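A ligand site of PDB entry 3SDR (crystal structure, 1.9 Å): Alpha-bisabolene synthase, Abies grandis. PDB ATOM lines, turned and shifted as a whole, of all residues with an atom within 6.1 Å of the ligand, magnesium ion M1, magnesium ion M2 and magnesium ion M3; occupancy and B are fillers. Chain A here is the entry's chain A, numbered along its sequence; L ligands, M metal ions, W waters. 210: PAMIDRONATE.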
ATOM      1  N   ARG A 531     -27.906  -9.133   7.793  1.00  0.00           N
ATOM      2  CA  ARG A 531     -28.826  -8.288   7.034  1.00  0.00           C
ATOM      3  C   ARG A 531     -29.628  -9.048   5.980  1.00  0.00           C
ATOM      4  O   ARG A 531     -29.783  -8.547   4.866  1.00  0.00           O
ATOM      5  CB  ARG A 531     -28.049  -7.172   6.323  1.00  0.00           C
ATOM      6  CG  ARG A 531     -27.232  -6.266   7.227  1.00  0.00           C
ATOM      7  CD  ARG A 531     -26.750  -5.054   6.461  1.00  0.00           C
ATOM      8  NE  ARG A 531     -25.500  -5.291   5.745  1.00  0.00           N
ATOM      9  CZ  ARG A 531     -25.128  -4.643   4.649  1.00  0.00           C
ATOM     10  NH1 ARG A 531     -25.938  -3.729   4.109  1.00  0.00           N
ATOM     11  NH2 ARG A 531     -23.968  -4.906   4.076  1.00  0.00           N
ATOM     12  N   ASP A 566     -16.740  -9.624   2.379  1.00  0.00           N
ATOM     13  CA  ASP A 566     -16.297  -8.241   2.314  1.00  0.00           C
ATOM     14  C   ASP A 566     -15.664  -7.801   3.632  1.00  0.00           C
ATOM     15  O   ASP A 566     -14.550  -7.274   3.652  1.00  0.00           O
ATOM     16  CB  ASP A 566     -17.474  -7.330   1.984  1.00  0.00           C
ATOM     17  CG  ASP A 566     -17.050  -5.904   1.825  1.00  0.00           C
ATOM     18  OD1 ASP A 566     -16.166  -5.661   0.978  1.00  0.00           O
ATOM     19  OD2 ASP A 566     -17.569  -5.049   2.557  1.00  0.00           O
ATOM     20  N   ASP A 567     -16.381  -8.007   4.735  1.00  0.00           N
ATOM     21  CA  ASP A 567     -15.864  -7.629   6.048  1.00  0.00           C
ATOM     22  C   ASP A 567     -14.562  -8.362   6.360  1.00  0.00           C
ATOM     23  O   ASP A 567     -13.668  -7.836   7.012  1.00  0.00           O
ATOM     24  CB  ASP A 567     -16.892  -7.875   7.145  1.00  0.00           C
ATOM     25  CG  ASP A 567     -18.079  -6.917   7.066  1.00  0.00           C
ATOM     26  OD1 ASP A 567     -18.041  -5.961   6.268  1.00  0.00           O
ATOM     27  OD2 ASP A 567     -19.054  -7.133   7.814  1.00  0.00           O
ATOM     28  N   ASP A 570     -11.671  -6.768   3.920  1.00  0.00           N
ATOM     29  CA  ASP A 570     -11.328  -5.348   4.055  1.00  0.00           C
ATOM     30  C   ASP A 570     -11.225  -4.865   5.511  1.00  0.00           C
ATOM     31  O   ASP A 570     -10.904  -3.710   5.749  1.00  0.00           O
ATOM     32  CB  ASP A 570     -12.249  -4.452   3.205  1.00  0.00           C
ATOM     33  CG  ASP A 570     -13.666  -4.395   3.718  1.00  0.00           C
ATOM     34  OD1 ASP A 570     -13.870  -4.625   4.925  1.00  0.00           O
ATOM     35  OD2 ASP A 570     -14.590  -4.100   2.912  1.00  0.00           O
ATOM     36  N   THR A 571     -11.473  -5.759   6.459  1.00  0.00           N
ATOM     37  CA  THR A 571     -11.474  -5.366   7.867  1.00  0.00           C
ATOM     38  C   THR A 571     -10.893  -6.425   8.804  1.00  0.00           C
ATOM     39  O   THR A 571      -9.826  -6.219   9.392  1.00  0.00           O
ATOM     40  CB  THR A 571     -12.893  -4.974   8.334  1.00  0.00           C
ATOM     41  OG1 THR A 571     -13.399  -3.918   7.509  1.00  0.00           O
ATOM     42  CG2 THR A 571     -12.865  -4.500   9.779  1.00  0.00           C
ATOM     43  N   TYR A 641     -10.792  -8.582  -4.145  1.00  0.00           N
ATOM     44  CA  TYR A 641     -10.704  -8.318  -2.714  1.00  0.00           C
ATOM     45  C   TYR A 641      -9.270  -8.400  -2.210  1.00  0.00           C
ATOM     46  O   TYR A 641      -8.842  -7.579  -1.395  1.00  0.00           O
ATOM     47  CB  TYR A 641     -11.543  -9.326  -1.915  1.00  0.00           C
ATOM     48  CG  TYR A 641     -12.995  -8.957  -1.732  1.00  0.00           C
ATOM     49  CD1 TYR A 641     -13.452  -7.683  -2.050  1.00  0.00           C
ATOM     50  CD2 TYR A 641     -13.909  -9.883  -1.235  1.00  0.00           C
ATOM     51  CE1 TYR A 641     -14.788  -7.349  -1.894  1.00  0.00           C
ATOM     52  CE2 TYR A 641     -15.243  -9.556  -1.072  1.00  0.00           C
ATOM     53  CZ  TYR A 641     -15.671  -8.290  -1.393  1.00  0.00           C
ATOM     54  OH  TYR A 641     -17.005  -7.963  -1.230  1.00  0.00           O
ATOM     55  N   GLU A 644      -7.117  -5.492  -3.084  1.00  0.00           N
ATOM     56  CA  GLU A 644      -7.523  -4.433  -2.178  1.00  0.00           C
ATOM     57  C   GLU A 644      -6.910  -4.634  -0.791  1.00  0.00           C
ATOM     58  O   GLU A 644      -6.494  -3.675  -0.138  1.00  0.00           O
ATOM     59  CB  GLU A 644      -9.048  -4.435  -2.069  1.00  0.00           C
ATOM     60  CG  GLU A 644      -9.682  -3.112  -1.695  1.00  0.00           C
ATOM     61  CD  GLU A 644     -11.198  -3.175  -1.780  1.00  0.00           C
ATOM     62  OE1 GLU A 644     -11.829  -2.137  -2.075  1.00  0.00           O
ATOM     63  OE2 GLU A 644     -11.759  -4.261  -1.565  1.00  0.00           O
ATOM     64  N   SER A 666     -14.199  -5.863  -7.621  1.00  0.00           N
ATOM     65  CA  SER A 666     -14.253  -6.221  -6.203  1.00  0.00           C
ATOM     66  C   SER A 666     -15.560  -5.801  -5.539  1.00  0.00           C
ATOM     67  O   SER A 666     -15.886  -6.296  -4.460  1.00  0.00           O
ATOM     68  CB  SER A 666     -13.058  -5.649  -5.440  1.00  0.00           C
ATOM     69  OG  SER A 666     -13.093  -4.240  -5.483  1.00  0.00           O
ATOM     70  N   ILE A 667     -16.325  -4.906  -6.152  1.00  0.00           N
ATOM     71  CA  ILE A 667     -17.569  -4.516  -5.494  1.00  0.00           C
ATOM     72  C   ILE A 667     -18.553  -5.681  -5.380  1.00  0.00           C
ATOM     73  O   ILE A 667     -19.439  -5.693  -4.518  1.00  0.00           O
ATOM     74  CB  ILE A 667     -18.239  -3.265  -6.108  1.00  0.00           C
ATOM     75  CG1 ILE A 667     -19.214  -2.674  -5.096  1.00  0.00           C
ATOM     76  CG2 ILE A 667     -18.916  -3.600  -7.430  1.00  0.00           C
ATOM     77  CD1 ILE A 667     -19.935  -1.483  -5.556  1.00  0.00           C
ATOM     78  N   GLY A 668     -18.388  -6.692  -6.235  1.00  0.00           N
ATOM     79  CA  GLY A 668     -19.135  -7.939  -6.103  1.00  0.00           C
ATOM     80  C   GLY A 668     -20.514  -7.978  -6.746  1.00  0.00           C
ATOM     81  O   GLY A 668     -21.216  -8.984  -6.635  1.00  0.00           O
ATOM     82  N   GLN A 669     -20.904  -6.891  -7.403  1.00  0.00           N
ATOM     83  CA  GLN A 669     -22.240  -6.833  -8.001  1.00  0.00           C
ATOM     84  C   GLN A 669     -22.351  -7.789  -9.173  1.00  0.00           C
ATOM     85  O   GLN A 669     -23.400  -8.371  -9.400  1.00  0.00           O
ATOM     86  CB  GLN A 669     -22.572  -5.409  -8.444  1.00  0.00           C
ATOM     87  CG  GLN A 669     -22.762  -4.463  -7.296  1.00  0.00           C
ATOM     88  CD  GLN A 669     -24.046  -4.724  -6.545  1.00  0.00           C
ATOM     89  OE1 GLN A 669     -24.037  -5.255  -5.424  1.00  0.00           O
ATOM     90  NE2 GLN A 669     -25.167  -4.382  -7.150  1.00  0.00           N
ATOM     91  N   ARG A 710     -20.244   1.068  -7.259  1.00  0.00           N
ATOM     92  CA  ARG A 710     -18.994   1.495  -6.629  1.00  0.00           C
ATOM     93  C   ARG A 710     -18.978   3.000  -6.396  1.00  0.00           C
ATOM     94  O   ARG A 710     -18.668   3.466  -5.297  1.00  0.00           O
ATOM     95  CB  ARG A 710     -17.793   1.073  -7.480  1.00  0.00           C
ATOM     96  CG  ARG A 710     -16.438   1.630  -7.002  1.00  0.00           C
ATOM     97  CD  ARG A 710     -15.962   0.948  -5.710  1.00  0.00           C
ATOM     98  NE  ARG A 710     -16.653   1.474  -4.529  1.00  0.00           N
ATOM     99  CZ  ARG A 710     -16.709   0.855  -3.356  1.00  0.00           C
ATOM    100  NH1 ARG A 710     -16.127  -0.327  -3.189  1.00  0.00           N
ATOM    101  NH2 ARG A 710     -17.367   1.415  -2.348  1.00  0.00           N
ATOM    102  N   ASP A 713     -21.896   4.451  -4.141  1.00  0.00           N
ATOM    103  CA  ASP A 713     -21.489   4.130  -2.782  1.00  0.00           C
ATOM    104  C   ASP A 713     -20.499   5.175  -2.263  1.00  0.00           C
ATOM    105  O   ASP A 713     -20.670   5.720  -1.161  1.00  0.00           O
ATOM    106  CB  ASP A 713     -20.862   2.733  -2.737  1.00  0.00           C
ATOM    107  CG  ASP A 713     -20.403   2.328  -1.345  1.00  0.00           C
ATOM    108  OD1 ASP A 713     -19.665   3.099  -0.701  1.00  0.00           O
ATOM    109  OD2 ASP A 713     -20.786   1.227  -0.911  1.00  0.00           O
ATOM    110  N   ASP A 714     -19.462   5.455  -3.043  1.00  0.00           N
ATOM    111  CA  ASP A 714     -18.444   6.422  -2.643  1.00  0.00           C
ATOM    112  C   ASP A 714     -19.038   7.810  -2.376  1.00  0.00           C
ATOM    113  O   ASP A 714     -18.697   8.440  -1.374  1.00  0.00           O
ATOM    114  CB  ASP A 714     -17.344   6.523  -3.699  1.00  0.00           C
ATOM    115  CG  ASP A 714     -16.451   5.290  -3.716  1.00  0.00           C
ATOM    116  OD1 ASP A 714     -16.687   4.390  -2.888  1.00  0.00           O
ATOM    117  OD2 ASP A 714     -15.513   5.235  -4.530  1.00  0.00           O
ATOM    118  N   THR A 717     -21.016   7.722   0.853  1.00  0.00           N
ATOM    119  CA  THR A 717     -20.213   7.428   2.028  1.00  0.00           C
ATOM    120  C   THR A 717     -18.859   8.125   1.917  1.00  0.00           C
ATOM    121  O   THR A 717     -18.804   9.337   1.767  1.00  0.00           O
ATOM    122  CB  THR A 717     -20.075   5.898   2.260  1.00  0.00           C
ATOM    123  OG1 THR A 717     -19.559   5.270   1.085  1.00  0.00           O
ATOM    124  CG2 THR A 717     -21.443   5.297   2.558  1.00  0.00           C
ATOM    125  N   TYR A 718     -17.768   7.372   1.975  1.00  0.00           N
ATOM    126  CA  TYR A 718     -16.427   7.964   1.802  1.00  0.00           C
ATOM    127  C   TYR A 718     -16.060   9.013   2.866  1.00  0.00           C
ATOM    128  O   TYR A 718     -14.904   9.083   3.291  1.00  0.00           O
ATOM    129  CB  TYR A 718     -16.231   8.527   0.384  1.00  0.00           C
ATOM    130  CG  TYR A 718     -16.237  10.046   0.293  1.00  0.00           C
ATOM    131  CD1 TYR A 718     -17.374  10.725  -0.147  1.00  0.00           C
ATOM    132  CD2 TYR A 718     -15.117  10.799   0.636  1.00  0.00           C
ATOM    133  CE1 TYR A 718     -17.394  12.100  -0.238  1.00  0.00           C
ATOM    134  CE2 TYR A 718     -15.128  12.179   0.546  1.00  0.00           C
ATOM    135  CZ  TYR A 718     -16.269  12.824   0.105  1.00  0.00           C
ATOM    136  OH  TYR A 718     -16.288  14.199   0.013  1.00  0.00           O
ATOM    137  N   PHE A 790     -28.304   4.707  -2.175  1.00  0.00           N
ATOM    138  CA  PHE A 790     -27.173   5.642  -2.211  1.00  0.00           C
ATOM    139  C   PHE A 790     -27.502   7.040  -2.734  1.00  0.00           C
ATOM    140  O   PHE A 790     -26.589   7.822  -3.029  1.00  0.00           O
ATOM    141  CB  PHE A 790     -26.031   5.045  -3.034  1.00  0.00           C
ATOM    142  CG  PHE A 790     -25.459   3.796  -2.455  1.00  0.00           C
ATOM    143  CD1 PHE A 790     -25.122   3.733  -1.106  1.00  0.00           C
ATOM    144  CD2 PHE A 790     -25.269   2.673  -3.238  1.00  0.00           C
ATOM    145  CE1 PHE A 790     -24.595   2.579  -0.566  1.00  0.00           C
ATOM    146  CE2 PHE A 790     -24.740   1.512  -2.692  1.00  0.00           C
ATOM    147  CZ  PHE A 790     -24.407   1.463  -1.356  1.00  0.00           C
HETATM  148  P1  210 L   1     -19.004  -1.317   2.836  1.00  0.00           P
HETATM  149  O2  210 L   1     -18.300   0.019   3.223  1.00  0.00           O
HETATM  150  O3  210 L   1     -20.537  -1.150   3.057  1.00  0.00           O
HETATM  151  O5  210 L   1     -18.461  -2.458   3.643  1.00  0.00           O
HETATM  152  C7  210 L   1     -18.710  -1.585   1.061  1.00  0.00           C
HETATM  153  P8  210 L   1     -16.908  -1.497   0.803  1.00  0.00           P
HETATM  154  O9  210 L   1     -16.258  -2.710   1.416  1.00  0.00           O
HETATM  155  O10 210 L   1     -16.434  -0.160   1.457  1.00  0.00           O
HETATM  156  O12 210 L   1     -16.640  -1.414  -0.721  1.00  0.00           O
HETATM  157  O14 210 L   1     -19.309  -0.598   0.326  1.00  0.00           O
HETATM  158  C16 210 L   1     -19.204  -2.952   0.690  1.00  0.00           C
HETATM  159  C19 210 L   1     -19.870  -2.944  -0.646  1.00  0.00           C
HETATM  160  N22 210 L   1     -20.273  -4.277  -0.988  1.00  0.00           N
HETATM  161 MG    MG M   1     -16.593  -3.282   3.214  1.00  0.00          MG
HETATM  162 MG    MG M   2     -17.962   1.684   2.108  1.00  0.00          MG
HETATM  163 MG    MG M   3     -14.881  -4.062   0.824  1.00  0.00          MG
HETATM  164  O   HOH W   1     -17.634  -5.606  -2.043  1.00  0.00           O
HETATM  165  O   HOH W   2     -16.591  -3.907   5.160  1.00  0.00           O
HETATM  166  O   HOH W   3     -22.008  -5.391  -3.767  1.00  0.00           O
HETATM  167  O   HOH W   4     -19.316   2.441   3.470  1.00  0.00           O
HETATM  168  O   HOH W   5     -15.624  -3.744  -1.064  1.00  0.00           O
HETATM  169  O   HOH W   6     -15.697  -1.473   3.796  1.00  0.00           O
HETATM  170  O   HOH W   7     -13.558  -2.473   0.539  1.00  0.00           O
HETATM  171  O   HOH W   8     -16.326   1.777   3.378  1.00  0.00           O
HETATM  172  O   HOH W   9     -13.535  -5.475   0.131  1.00  0.00           O
HETATM  173  O   HOH W  10     -16.937   2.384   0.453  1.00  0.00           O
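Magnesium ion M2 is bound by an oxygen (O2) of the ligand (2.0 Å), water W4 (2.1 Å), water W10 (2.1 Å), water W8 (2.1 Å) and an oxygen (O10) of the ligand (2.5 Å). Magnesium ion M2 has five donor atoms within binding distance.
Merely in contact with the ligand: Ile 667 (3.9 Å). Of the 17 residues printed, 5 come within 4 Å of the ligand.
Magnesium ion M3 is bound by O9 of the ligand (2.0 Å), water W5 (2.1 Å), OD1 of Asp 566 (2.1 Å), water W9 (2.1 Å), water W7 (2.1 Å) and OD2 of Asp 570 (2.1 Å). Magnesium ion M3 has six donor atoms within binding distance.
Merely in contact with magnesium ion M2: Asp 713. Of the 17 residues printed, 1 comes within 4 Å of magnesium ion M2.
The side-chain carboxylate (OD1) of Asp 566 lies close to the side-chain hydroxyl (OH) of Tyr 641 (3.3 Å). OD1 of Asp 570 sits at hydrogen-bond distance from OG1 of Thr 571 (2.7 Å). The side-chain carboxylate (OD1) of Asp 713 is in salt-bridge range of the guanidinium group (NH2) of Arg 710, 3.3 Å away. O of Asp 713 sits at hydrogen-bond distance from OG1 of Thr 717 (2.5 Å). The side-chain carboxylate (OD1) of Asp 714 is in salt-bridge range of the guanidinium group (NH2) of Arg 710.
The side-chain carboxylate (OD2) of Asp 713 lies within hydrogen-bond range of an oxygen (O14) of the ligand, 2.7 Å away. An oxygen (O12) of the ligand is in salt-bridge range of the guanidinium group (NH1) of Arg 710.
Of the 17 residues printed, 2 come within 4 Å of magnesium ion M1. The nearest printed residue that does not touch magnesium ion M1 is Asp 567 (4.3 Å).
Magnesium ion M1 is bound by an oxygen (O9) of the ligand (1.9 Å), water W2 (2.0 Å), an oxygen (O5) of the ligand (2.1 Å), water W6 (2.1 Å), the side-chain carboxylate of Asp 566 (2.1 Å) and the side-chain carboxylate of Asp 570 (2.2 Å).
Water W2 bridges the side-chain carboxylate of Asp 567 and the side-chain carboxylate of Asp 570. Water W10 lies within hydrogen-bond range of NH2 of Arg 710 (3.0 Å) and OD1 of Asp 713 (3.0 Å). Water W7 lies within hydrogen-bond range of the side-chain carboxylate (OE1) of Glu 644 (3.2 Å) and an oxygen (O12) of the ligand (3.5 Å). Water W1 lies within hydrogen-bond range of the side-chain hydroxyl of Tyr 641 (2.6 Å), the backbone carbonyl oxygen of Ser 666 (3.1 Å), the backbone carbonyl oxygen of Ile 667 (3.1 Å) and a nitrogen (N22) of the ligand (3.1 Å). Water W3 lies within hydrogen-bond range of the side-chain amide oxygen (OE1) of Gln 669 (2.6 Å), the backbone carbonyl oxygen (O) of Ile 667 (2.7 Å) and a nitrogen (N22) of the ligand (3.5 Å).
Glu 644 touches magnesium ion M3. Within 4 Å of magnesium ion M3: Asp 566, Asp 570 and Glu 644. The nearest printed residue that does not touch magnesium ion M3 is Tyr 641 (4.3 Å).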
